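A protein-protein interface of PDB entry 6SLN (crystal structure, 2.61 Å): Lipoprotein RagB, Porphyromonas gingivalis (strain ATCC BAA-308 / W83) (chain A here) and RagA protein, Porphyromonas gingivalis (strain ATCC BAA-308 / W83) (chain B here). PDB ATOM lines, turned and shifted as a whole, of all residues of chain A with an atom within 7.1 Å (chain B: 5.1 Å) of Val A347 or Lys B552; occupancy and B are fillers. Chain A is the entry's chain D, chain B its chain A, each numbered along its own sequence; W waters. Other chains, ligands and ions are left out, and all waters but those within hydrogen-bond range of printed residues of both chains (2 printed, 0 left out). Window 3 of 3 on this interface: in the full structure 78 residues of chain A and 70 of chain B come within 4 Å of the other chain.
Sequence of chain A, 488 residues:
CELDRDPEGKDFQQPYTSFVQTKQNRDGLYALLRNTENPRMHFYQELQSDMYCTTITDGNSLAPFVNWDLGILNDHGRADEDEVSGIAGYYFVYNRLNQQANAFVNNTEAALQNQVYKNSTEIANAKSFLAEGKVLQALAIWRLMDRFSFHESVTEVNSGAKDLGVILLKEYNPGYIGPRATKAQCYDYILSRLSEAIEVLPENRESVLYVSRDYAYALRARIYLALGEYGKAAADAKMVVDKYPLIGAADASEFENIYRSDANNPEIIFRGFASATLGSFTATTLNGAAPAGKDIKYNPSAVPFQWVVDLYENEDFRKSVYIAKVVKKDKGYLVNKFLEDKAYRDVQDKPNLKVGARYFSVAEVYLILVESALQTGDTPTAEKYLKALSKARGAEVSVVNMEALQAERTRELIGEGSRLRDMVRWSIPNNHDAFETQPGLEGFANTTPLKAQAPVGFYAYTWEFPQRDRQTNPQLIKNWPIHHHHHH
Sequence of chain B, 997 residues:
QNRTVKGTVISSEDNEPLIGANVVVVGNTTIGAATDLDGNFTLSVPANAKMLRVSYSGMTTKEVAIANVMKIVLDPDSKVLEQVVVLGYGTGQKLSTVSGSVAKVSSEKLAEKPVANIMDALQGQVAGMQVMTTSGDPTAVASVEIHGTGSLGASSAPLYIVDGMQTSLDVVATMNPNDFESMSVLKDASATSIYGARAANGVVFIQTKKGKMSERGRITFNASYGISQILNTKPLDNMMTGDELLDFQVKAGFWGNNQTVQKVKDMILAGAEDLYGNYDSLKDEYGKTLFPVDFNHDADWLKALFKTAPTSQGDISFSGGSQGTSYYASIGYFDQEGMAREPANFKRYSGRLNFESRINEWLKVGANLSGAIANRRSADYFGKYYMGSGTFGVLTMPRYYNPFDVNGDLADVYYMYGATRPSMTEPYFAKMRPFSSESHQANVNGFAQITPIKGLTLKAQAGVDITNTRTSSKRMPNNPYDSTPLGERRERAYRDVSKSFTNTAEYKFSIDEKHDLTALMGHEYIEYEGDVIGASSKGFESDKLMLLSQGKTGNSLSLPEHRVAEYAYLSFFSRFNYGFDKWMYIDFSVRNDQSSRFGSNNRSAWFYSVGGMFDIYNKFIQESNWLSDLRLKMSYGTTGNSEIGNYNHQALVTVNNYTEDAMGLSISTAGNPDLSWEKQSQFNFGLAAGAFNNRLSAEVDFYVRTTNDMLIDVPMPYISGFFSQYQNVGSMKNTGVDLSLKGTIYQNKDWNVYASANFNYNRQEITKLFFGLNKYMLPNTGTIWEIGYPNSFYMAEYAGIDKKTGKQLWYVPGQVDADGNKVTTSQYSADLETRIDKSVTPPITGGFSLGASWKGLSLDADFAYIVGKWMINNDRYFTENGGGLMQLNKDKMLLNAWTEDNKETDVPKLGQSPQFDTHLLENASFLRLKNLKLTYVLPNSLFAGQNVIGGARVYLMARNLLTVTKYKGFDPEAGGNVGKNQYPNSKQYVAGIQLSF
NZ of Lys B538 is in salt-bridge range of OD2 of Asp A346 (2.8 Å).
The backbone NH of Lys B552 lies within hydrogen-bond range of the backbone carbonyl oxygen of Lys B538, at 3.0 Å.
The backbone carbonyl oxygen of Gly B539 is in hydrogen-bond range of the side-chain amino group of Lys B552, 2.7 Å away.
OE1 of Glu B541 lies within salt-bridge range of NZ of Lys B552, 2.5 Å away.
ND2 of Asn A352 is in hydrogen-bond range of OD1 of Asp A346 (3.2 Å).
Among the printed residues, merely in contact across the chains: Lys A350 with Leu B486 (3.4 Å), Val A347 with Leu B486 (3.6 Å), Val A347 with Lys B552 (3.7 Å), Asp A346 with Ser B556 (3.7 Å) and Val A347 with Ser B556 (3.9 Å).
Val A347 touches just these residues of chain B: Leu B486 (3.6 Å), Lys B552 (3.7 Å) and Ser B556 (3.9 Å).
Lys B552 touches one residue of chain A.
Of the printed residues of chain A, Ser B556 touches Asp A346 (3.7 Å) and Val A347 (3.9 Å).
Of the printed residues of chain B, Lys A350 touches Leu B486 (3.4 Å).
Printed residues of chain A within 4 Å of Lys B538: Asp A346 (2.8 Å).
Of the printed residues of chain A, Leu B486 touches Val A347 and Lys A350.
The nearest printed residue of chain A that does not touch Ser B556 is Arg A345 (5.9 Å).
Of the 10 printed residues of chain A, 3 touch a printed residue of chain B.
Hydrophobic or aromatic side chains of chain A within 4 Å of the printed part of chain B: Val A347.
Hydrophobic or aromatic side chains of chain B within 4 Å of the printed part of chain A: Leu B486.
Among the printed residues, 6 pairs touch across the chains.
Among the printed residues, Asp or Glu carboxylates within 4 Å of a Lys or Arg side-chain nitrogen of the other chain: Asp A346 with Lys B538.
Water W2 lies within hydrogen-bond range of OG of Ser B556 (2.5 Å), O of Asp A346 (2.8 Å) and O of Thr B553 (3.2 Å).
Water W1 lies within hydrogen-bond range of O of Leu B557, NZ of Lys B538 and OD2 of Asp A346.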
ATOM      1  N   LYS A 342       8.549 -38.086 -12.495  1.00  0.00           N
ATOM      2  CA  LYS A 342       7.638 -36.954 -12.698  1.00  0.00           C
ATOM      3  C   LYS A 342       6.423 -37.037 -11.772  1.00  0.00           C
ATOM      4  O   LYS A 342       5.877 -36.006 -11.367  1.00  0.00           O
ATOM      5  CB  LYS A 342       7.193 -36.874 -14.162  1.00  0.00           C
ATOM      6  CG  LYS A 342       8.289 -36.501 -15.144  1.00  0.00           C
ATOM      7  CD  LYS A 342       7.837 -36.677 -16.588  1.00  0.00           C
ATOM      8  CE  LYS A 342       8.890 -36.191 -17.566  1.00  0.00           C
ATOM      9  NZ  LYS A 342       8.395 -36.314 -18.959  1.00  0.00           N
ATOM     10  N   TYR A 344       6.259 -37.311  -8.766  1.00  0.00           N
ATOM     11  CA  TYR A 344       6.454 -36.685  -7.465  1.00  0.00           C
ATOM     12  C   TYR A 344       6.498 -35.165  -7.557  1.00  0.00           C
ATOM     13  O   TYR A 344       6.783 -34.491  -6.558  1.00  0.00           O
ATOM     14  CB  TYR A 344       7.723 -37.249  -6.800  1.00  0.00           C
ATOM     15  CG  TYR A 344       7.687 -38.765  -6.667  1.00  0.00           C
ATOM     16  CD1 TYR A 344       6.485 -39.425  -6.437  1.00  0.00           C
ATOM     17  CD2 TYR A 344       8.844 -39.538  -6.783  1.00  0.00           C
ATOM     18  CE1 TYR A 344       6.427 -40.798  -6.340  1.00  0.00           C
ATOM     19  CE2 TYR A 344       8.793 -40.923  -6.688  1.00  0.00           C
ATOM     20  CZ  TYR A 344       7.581 -41.544  -6.465  1.00  0.00           C
ATOM     21  OH  TYR A 344       7.491 -42.906  -6.355  1.00  0.00           O
ATOM     22  N   ARG A 345       6.215 -34.606  -8.731  1.00  0.00           N
ATOM     23  CA  ARG A 345       6.232 -33.161  -8.868  1.00  0.00           C
ATOM     24  C   ARG A 345       5.053 -32.542  -8.123  1.00  0.00           C
ATOM     25  O   ARG A 345       3.980 -33.138  -8.004  1.00  0.00           O
ATOM     26  CB  ARG A 345       6.172 -32.760 -10.337  1.00  0.00           C
ATOM     27  CG  ARG A 345       7.339 -33.222 -11.173  1.00  0.00           C
ATOM     28  CD  ARG A 345       7.137 -32.845 -12.619  1.00  0.00           C
ATOM     29  NE  ARG A 345       8.383 -32.884 -13.375  1.00  0.00           N
ATOM     30  CZ  ARG A 345       8.466 -32.557 -14.662  1.00  0.00           C
ATOM     31  NH1 ARG A 345       7.384 -32.171 -15.313  1.00  0.00           N
ATOM     32  NH2 ARG A 345       9.619 -32.616 -15.302  1.00  0.00           N
ATOM     33  N   ASP A 346       5.260 -31.322  -7.629  1.00  0.00           N
ATOM     34  CA  ASP A 346       4.144 -30.566  -7.074  1.00  0.00           C
ATOM     35  C   ASP A 346       3.211 -30.105  -8.181  1.00  0.00           C
ATOM     36  O   ASP A 346       2.004 -30.339  -8.134  1.00  0.00           O
ATOM     37  CB  ASP A 346       4.672 -29.391  -6.252  1.00  0.00           C
ATOM     38  CG  ASP A 346       5.544 -29.853  -5.079  1.00  0.00           C
ATOM     39  OD1 ASP A 346       5.851 -31.068  -4.984  1.00  0.00           O
ATOM     40  OD2 ASP A 346       5.924 -29.011  -4.246  1.00  0.00           O
ATOM     41  N   VAL A 347       3.758 -29.482  -9.209  1.00  0.00           N
ATOM     42  CA  VAL A 347       2.988 -29.079 -10.373  1.00  0.00           C
ATOM     43  C   VAL A 347       3.557 -29.831 -11.564  1.00  0.00           C
ATOM     44  O   VAL A 347       4.780 -29.907 -11.721  1.00  0.00           O
ATOM     45  CB  VAL A 347       3.032 -27.555 -10.565  1.00  0.00           C
ATOM     46  CG1 VAL A 347       2.243 -27.150 -11.788  1.00  0.00           C
ATOM     47  CG2 VAL A 347       2.482 -26.879  -9.334  1.00  0.00           C
ATOM     48  N   GLN A 348       2.674 -30.440 -12.361  1.00  0.00           N
ATOM     49  CA  GLN A 348       3.122 -31.303 -13.453  1.00  0.00           C
ATOM     50  C   GLN A 348       4.086 -30.576 -14.381  1.00  0.00           C
ATOM     51  O   GLN A 348       4.995 -31.189 -14.943  1.00  0.00           O
ATOM     52  CB  GLN A 348       1.914 -31.804 -14.242  1.00  0.00           C
ATOM     53  CG  GLN A 348       1.168 -32.942 -13.666  1.00  0.00           C
ATOM     54  CD  GLN A 348       0.145 -33.452 -14.656  1.00  0.00           C
ATOM     55  OE1 GLN A 348       0.360 -33.357 -15.863  1.00  0.00           O
ATOM     56  NE2 GLN A 348      -0.982 -33.971 -14.159  1.00  0.00           N
ATOM     57  N   ASP A 349       3.873 -29.266 -14.566  1.00  0.00           N
ATOM     58  CA  ASP A 349       4.740 -28.422 -15.388  1.00  0.00           C
ATOM     59  C   ASP A 349       6.178 -28.404 -14.874  1.00  0.00           C
ATOM     60  O   ASP A 349       7.133 -28.329 -15.659  1.00  0.00           O
ATOM     61  CB  ASP A 349       4.201 -26.986 -15.376  1.00  0.00           C
ATOM     62  CG  ASP A 349       3.651 -26.570 -16.672  1.00  0.00           C
ATOM     63  OD1 ASP A 349       3.980 -27.237 -17.670  1.00  0.00           O
ATOM     64  OD2 ASP A 349       2.889 -25.577 -16.699  1.00  0.00           O
ATOM     65  N   LYS A 350       6.347 -28.389 -13.557  1.00  0.00           N
ATOM     66  CA  LYS A 350       7.573 -27.905 -12.963  1.00  0.00           C
ATOM     67  C   LYS A 350       8.383 -29.073 -12.435  1.00  0.00           C
ATOM     68  O   LYS A 350       7.936 -29.758 -11.501  1.00  0.00           O
ATOM     69  CB  LYS A 350       7.269 -26.921 -11.836  1.00  0.00           C
ATOM     70  CG  LYS A 350       6.168 -25.906 -12.138  1.00  0.00           C
ATOM     71  CD  LYS A 350       6.452 -25.104 -13.413  1.00  0.00           C
ATOM     72  CE  LYS A 350       5.311 -24.164 -13.733  1.00  0.00           C
ATOM     73  NZ  LYS A 350       5.205 -23.205 -12.617  1.00  0.00           N
ATOM     74  N   PRO A 351       9.555 -29.346 -12.994  1.00  0.00           N
ATOM     75  CA  PRO A 351      10.449 -30.317 -12.364  1.00  0.00           C
ATOM     76  C   PRO A 351      10.777 -29.878 -10.949  1.00  0.00           C
ATOM     77  O   PRO A 351      11.047 -28.700 -10.700  1.00  0.00           O
ATOM     78  CB  PRO A 351      11.693 -30.297 -13.262  1.00  0.00           C
ATOM     79  CG  PRO A 351      11.234 -29.724 -14.552  1.00  0.00           C
ATOM     80  CD  PRO A 351      10.109 -28.790 -14.242  1.00  0.00           C
ATOM     81  N   ASN A 352      10.710 -30.835 -10.015  1.00  0.00           N
ATOM     82  CA  ASN A 352      11.320 -30.670  -8.711  1.00  0.00           C
ATOM     83  C   ASN A 352      12.345 -31.758  -8.434  1.00  0.00           C
ATOM     84  O   ASN A 352      12.893 -31.807  -7.319  1.00  0.00           O
ATOM     85  CB  ASN A 352      10.264 -30.630  -7.592  1.00  0.00           C
ATOM     86  CG  ASN A 352       9.371 -31.856  -7.564  1.00  0.00           C
ATOM     87  OD1 ASN A 352       9.462 -32.744  -8.424  1.00  0.00           O
ATOM     88  ND2 ASN A 352       8.471 -31.902  -6.578  1.00  0.00           N
ATOM     89  N   LEU B 486       6.347 -20.053  -9.293  1.00  0.00           N
ATOM     90  CA  LEU B 486       5.306 -20.188  -8.288  1.00  0.00           C
ATOM     91  C   LEU B 486       5.837 -19.665  -6.964  1.00  0.00           C
ATOM     92  O   LEU B 486       6.976 -19.942  -6.596  1.00  0.00           O
ATOM     93  CB  LEU B 486       4.868 -21.647  -8.177  1.00  0.00           C
ATOM     94  CG  LEU B 486       4.347 -22.118  -9.541  1.00  0.00           C
ATOM     95  CD1 LEU B 486       3.803 -23.555  -9.521  1.00  0.00           C
ATOM     96  CD2 LEU B 486       3.310 -21.121 -10.038  1.00  0.00           C
ATOM     97  N   LYS B 538       2.036 -22.979  -1.229  1.00  0.00           N
ATOM     98  CA  LYS B 538       2.864 -22.602  -2.356  1.00  0.00           C
ATOM     99  C   LYS B 538       2.070 -22.682  -3.652  1.00  0.00           C
ATOM    100  O   LYS B 538       0.910 -23.110  -3.684  1.00  0.00           O
ATOM    101  CB  LYS B 538       4.138 -23.457  -2.408  1.00  0.00           C
ATOM    102  CG  LYS B 538       3.932 -24.927  -2.259  1.00  0.00           C
ATOM    103  CD  LYS B 538       5.260 -25.622  -2.256  1.00  0.00           C
ATOM    104  CE  LYS B 538       5.050 -27.120  -2.067  1.00  0.00           C
ATOM    105  NZ  LYS B 538       6.290 -27.869  -1.700  1.00  0.00           N
ATOM    106  N   GLY B 539       2.725 -22.237  -4.723  1.00  0.00           N
ATOM    107  CA  GLY B 539       2.136 -22.253  -6.036  1.00  0.00           C
ATOM    108  C   GLY B 539       1.323 -21.032  -6.368  1.00  0.00           C
ATOM    109  O   GLY B 539       0.511 -21.093  -7.301  1.00  0.00           O
ATOM    110  N   PHE B 540       1.494 -19.942  -5.613  1.00  0.00           N
ATOM    111  CA  PHE B 540       0.899 -18.659  -5.964  1.00  0.00           C
ATOM    112  C   PHE B 540       1.433 -18.196  -7.310  1.00  0.00           C
ATOM    113  O   PHE B 540       2.609 -18.388  -7.624  1.00  0.00           O
ATOM    114  CB  PHE B 540       1.229 -17.617  -4.893  1.00  0.00           C
ATOM    115  CG  PHE B 540       0.879 -18.044  -3.490  1.00  0.00           C
ATOM    116  CD1 PHE B 540      -0.448 -18.205  -3.111  1.00  0.00           C
ATOM    117  CD2 PHE B 540       1.876 -18.305  -2.552  1.00  0.00           C
ATOM    118  CE1 PHE B 540      -0.781 -18.598  -1.822  1.00  0.00           C
ATOM    119  CE2 PHE B 540       1.552 -18.700  -1.256  1.00  0.00           C
ATOM    120  CZ  PHE B 540       0.217 -18.845  -0.893  1.00  0.00           C
ATOM    121  N   GLU B 541       0.571 -17.590  -8.122  1.00  0.00           N
ATOM    122  CA  GLU B 541       1.011 -17.045  -9.404  1.00  0.00           C
ATOM    123  C   GLU B 541       0.921 -15.536  -9.438  1.00  0.00           C
ATOM    124  O   GLU B 541       1.151 -14.930 -10.491  1.00  0.00           O
ATOM    125  CB  GLU B 541       0.223 -17.653 -10.564  1.00  0.00           C
ATOM    126  CG  GLU B 541       0.728 -19.021 -10.930  1.00  0.00           C
ATOM    127  CD  GLU B 541      -0.261 -19.868 -11.701  1.00  0.00           C
ATOM    128  OE1 GLU B 541      -0.193 -21.111 -11.581  1.00  0.00           O
ATOM    129  OE2 GLU B 541      -1.086 -19.306 -12.449  1.00  0.00           O
ATOM    130  N   GLN B 550      -4.984 -19.702  -0.488  1.00  0.00           N
ATOM    131  CA  GLN B 550      -5.050 -19.568  -1.931  1.00  0.00           C
ATOM    132  C   GLN B 550      -3.958 -20.342  -2.626  1.00  0.00           C
ATOM    133  O   GLN B 550      -3.716 -20.118  -3.821  1.00  0.00           O
ATOM    134  CB  GLN B 550      -5.007 -18.090  -2.314  1.00  0.00           C
ATOM    135  CG  GLN B 550      -6.133 -17.290  -1.651  1.00  0.00           C
ATOM    136  CD  GLN B 550      -6.190 -15.843  -2.096  1.00  0.00           C
ATOM    137  OE1 GLN B 550      -5.273 -15.043  -1.834  1.00  0.00           O
ATOM    138  NE2 GLN B 550      -7.272 -15.495  -2.775  1.00  0.00           N
ATOM    139  N   GLY B 551      -3.298 -21.249  -1.912  1.00  0.00           N
ATOM    140  CA  GLY B 551      -2.293 -22.080  -2.532  1.00  0.00           C
ATOM    141  C   GLY B 551      -2.877 -23.140  -3.451  1.00  0.00           C
ATOM    142  O   GLY B 551      -4.077 -23.446  -3.449  1.00  0.00           O
ATOM    143  N   LYS B 552      -1.996 -23.709  -4.269  1.00  0.00           N
ATOM    144  CA  LYS B 552      -2.361 -24.891  -5.031  1.00  0.00           C
ATOM    145  C   LYS B 552      -2.559 -26.038  -4.055  1.00  0.00           C
ATOM    146  O   LYS B 552      -1.991 -26.048  -2.963  1.00  0.00           O
ATOM    147  CB  LYS B 552      -1.287 -25.230  -6.086  1.00  0.00           C
ATOM    148  CG  LYS B 552      -0.910 -24.052  -7.012  1.00  0.00           C
ATOM    149  CD  LYS B 552      -0.135 -24.492  -8.249  1.00  0.00           C
ATOM    150  CE  LYS B 552      -0.623 -23.799  -9.542  1.00  0.00           C
ATOM    151  NZ  LYS B 552      -0.727 -22.323  -9.423  1.00  0.00           N
ATOM    152  N   THR B 553      -3.416 -26.977  -4.425  1.00  0.00           N
ATOM    153  CA  THR B 553      -3.657 -28.102  -3.537  1.00  0.00           C
ATOM    154  C   THR B 553      -2.866 -29.305  -4.026  1.00  0.00           C
ATOM    155  O   THR B 553      -1.800 -29.136  -4.631  1.00  0.00           O
ATOM    156  CB  THR B 553      -5.159 -28.417  -3.431  1.00  0.00           C
ATOM    157  OG1 THR B 553      -5.730 -28.687  -4.722  1.00  0.00           O
ATOM    158  CG2 THR B 553      -5.896 -27.274  -2.759  1.00  0.00           C
ATOM    159  N   GLY B 554      -3.379 -30.512  -3.773  1.00  0.00           N
ATOM    160  CA  GLY B 554      -2.729 -31.738  -4.213  1.00  0.00           C
ATOM    161  C   GLY B 554      -1.276 -31.789  -3.797  1.00  0.00           C
ATOM    162  O   GLY B 554      -0.909 -31.461  -2.658  1.00  0.00           O
ATOM    163  N   SER B 556       1.031 -29.890  -3.999  1.00  0.00           N
ATOM    164  CA  SER B 556       1.601 -28.660  -3.472  1.00  0.00           C
ATOM    165  C   SER B 556       1.306 -28.463  -1.985  1.00  0.00           C
ATOM    166  O   SER B 556       1.681 -27.429  -1.423  1.00  0.00           O
ATOM    167  CB  SER B 556       1.067 -27.457  -4.264  1.00  0.00           C
ATOM    168  OG  SER B 556       1.523 -27.464  -5.609  1.00  0.00           O
ATOM    169  N   LEU B 557       0.630 -29.400  -1.334  1.00  0.00           N
ATOM    170  CA  LEU B 557       0.284 -29.187   0.064  1.00  0.00           C
ATOM    171  C   LEU B 557       1.399 -29.693   0.969  1.00  0.00           C
ATOM    172  O   LEU B 557       2.394 -30.260   0.520  1.00  0.00           O
ATOM    173  CB  LEU B 557      -1.040 -29.871   0.404  1.00  0.00           C
ATOM    174  CG  LEU B 557      -2.180 -29.325  -0.445  1.00  0.00           C
ATOM    175  CD1 LEU B 557      -3.293 -30.347  -0.634  1.00  0.00           C
ATOM    176  CD2 LEU B 557      -2.696 -28.059   0.212  1.00  0.00           C
HETATM  177  O   HOH W   1       4.459 -30.317  -1.622  1.00  0.00           O
HETATM  178  O   HOH W   2       0.034 -28.594  -7.214  1.00  0.00           O
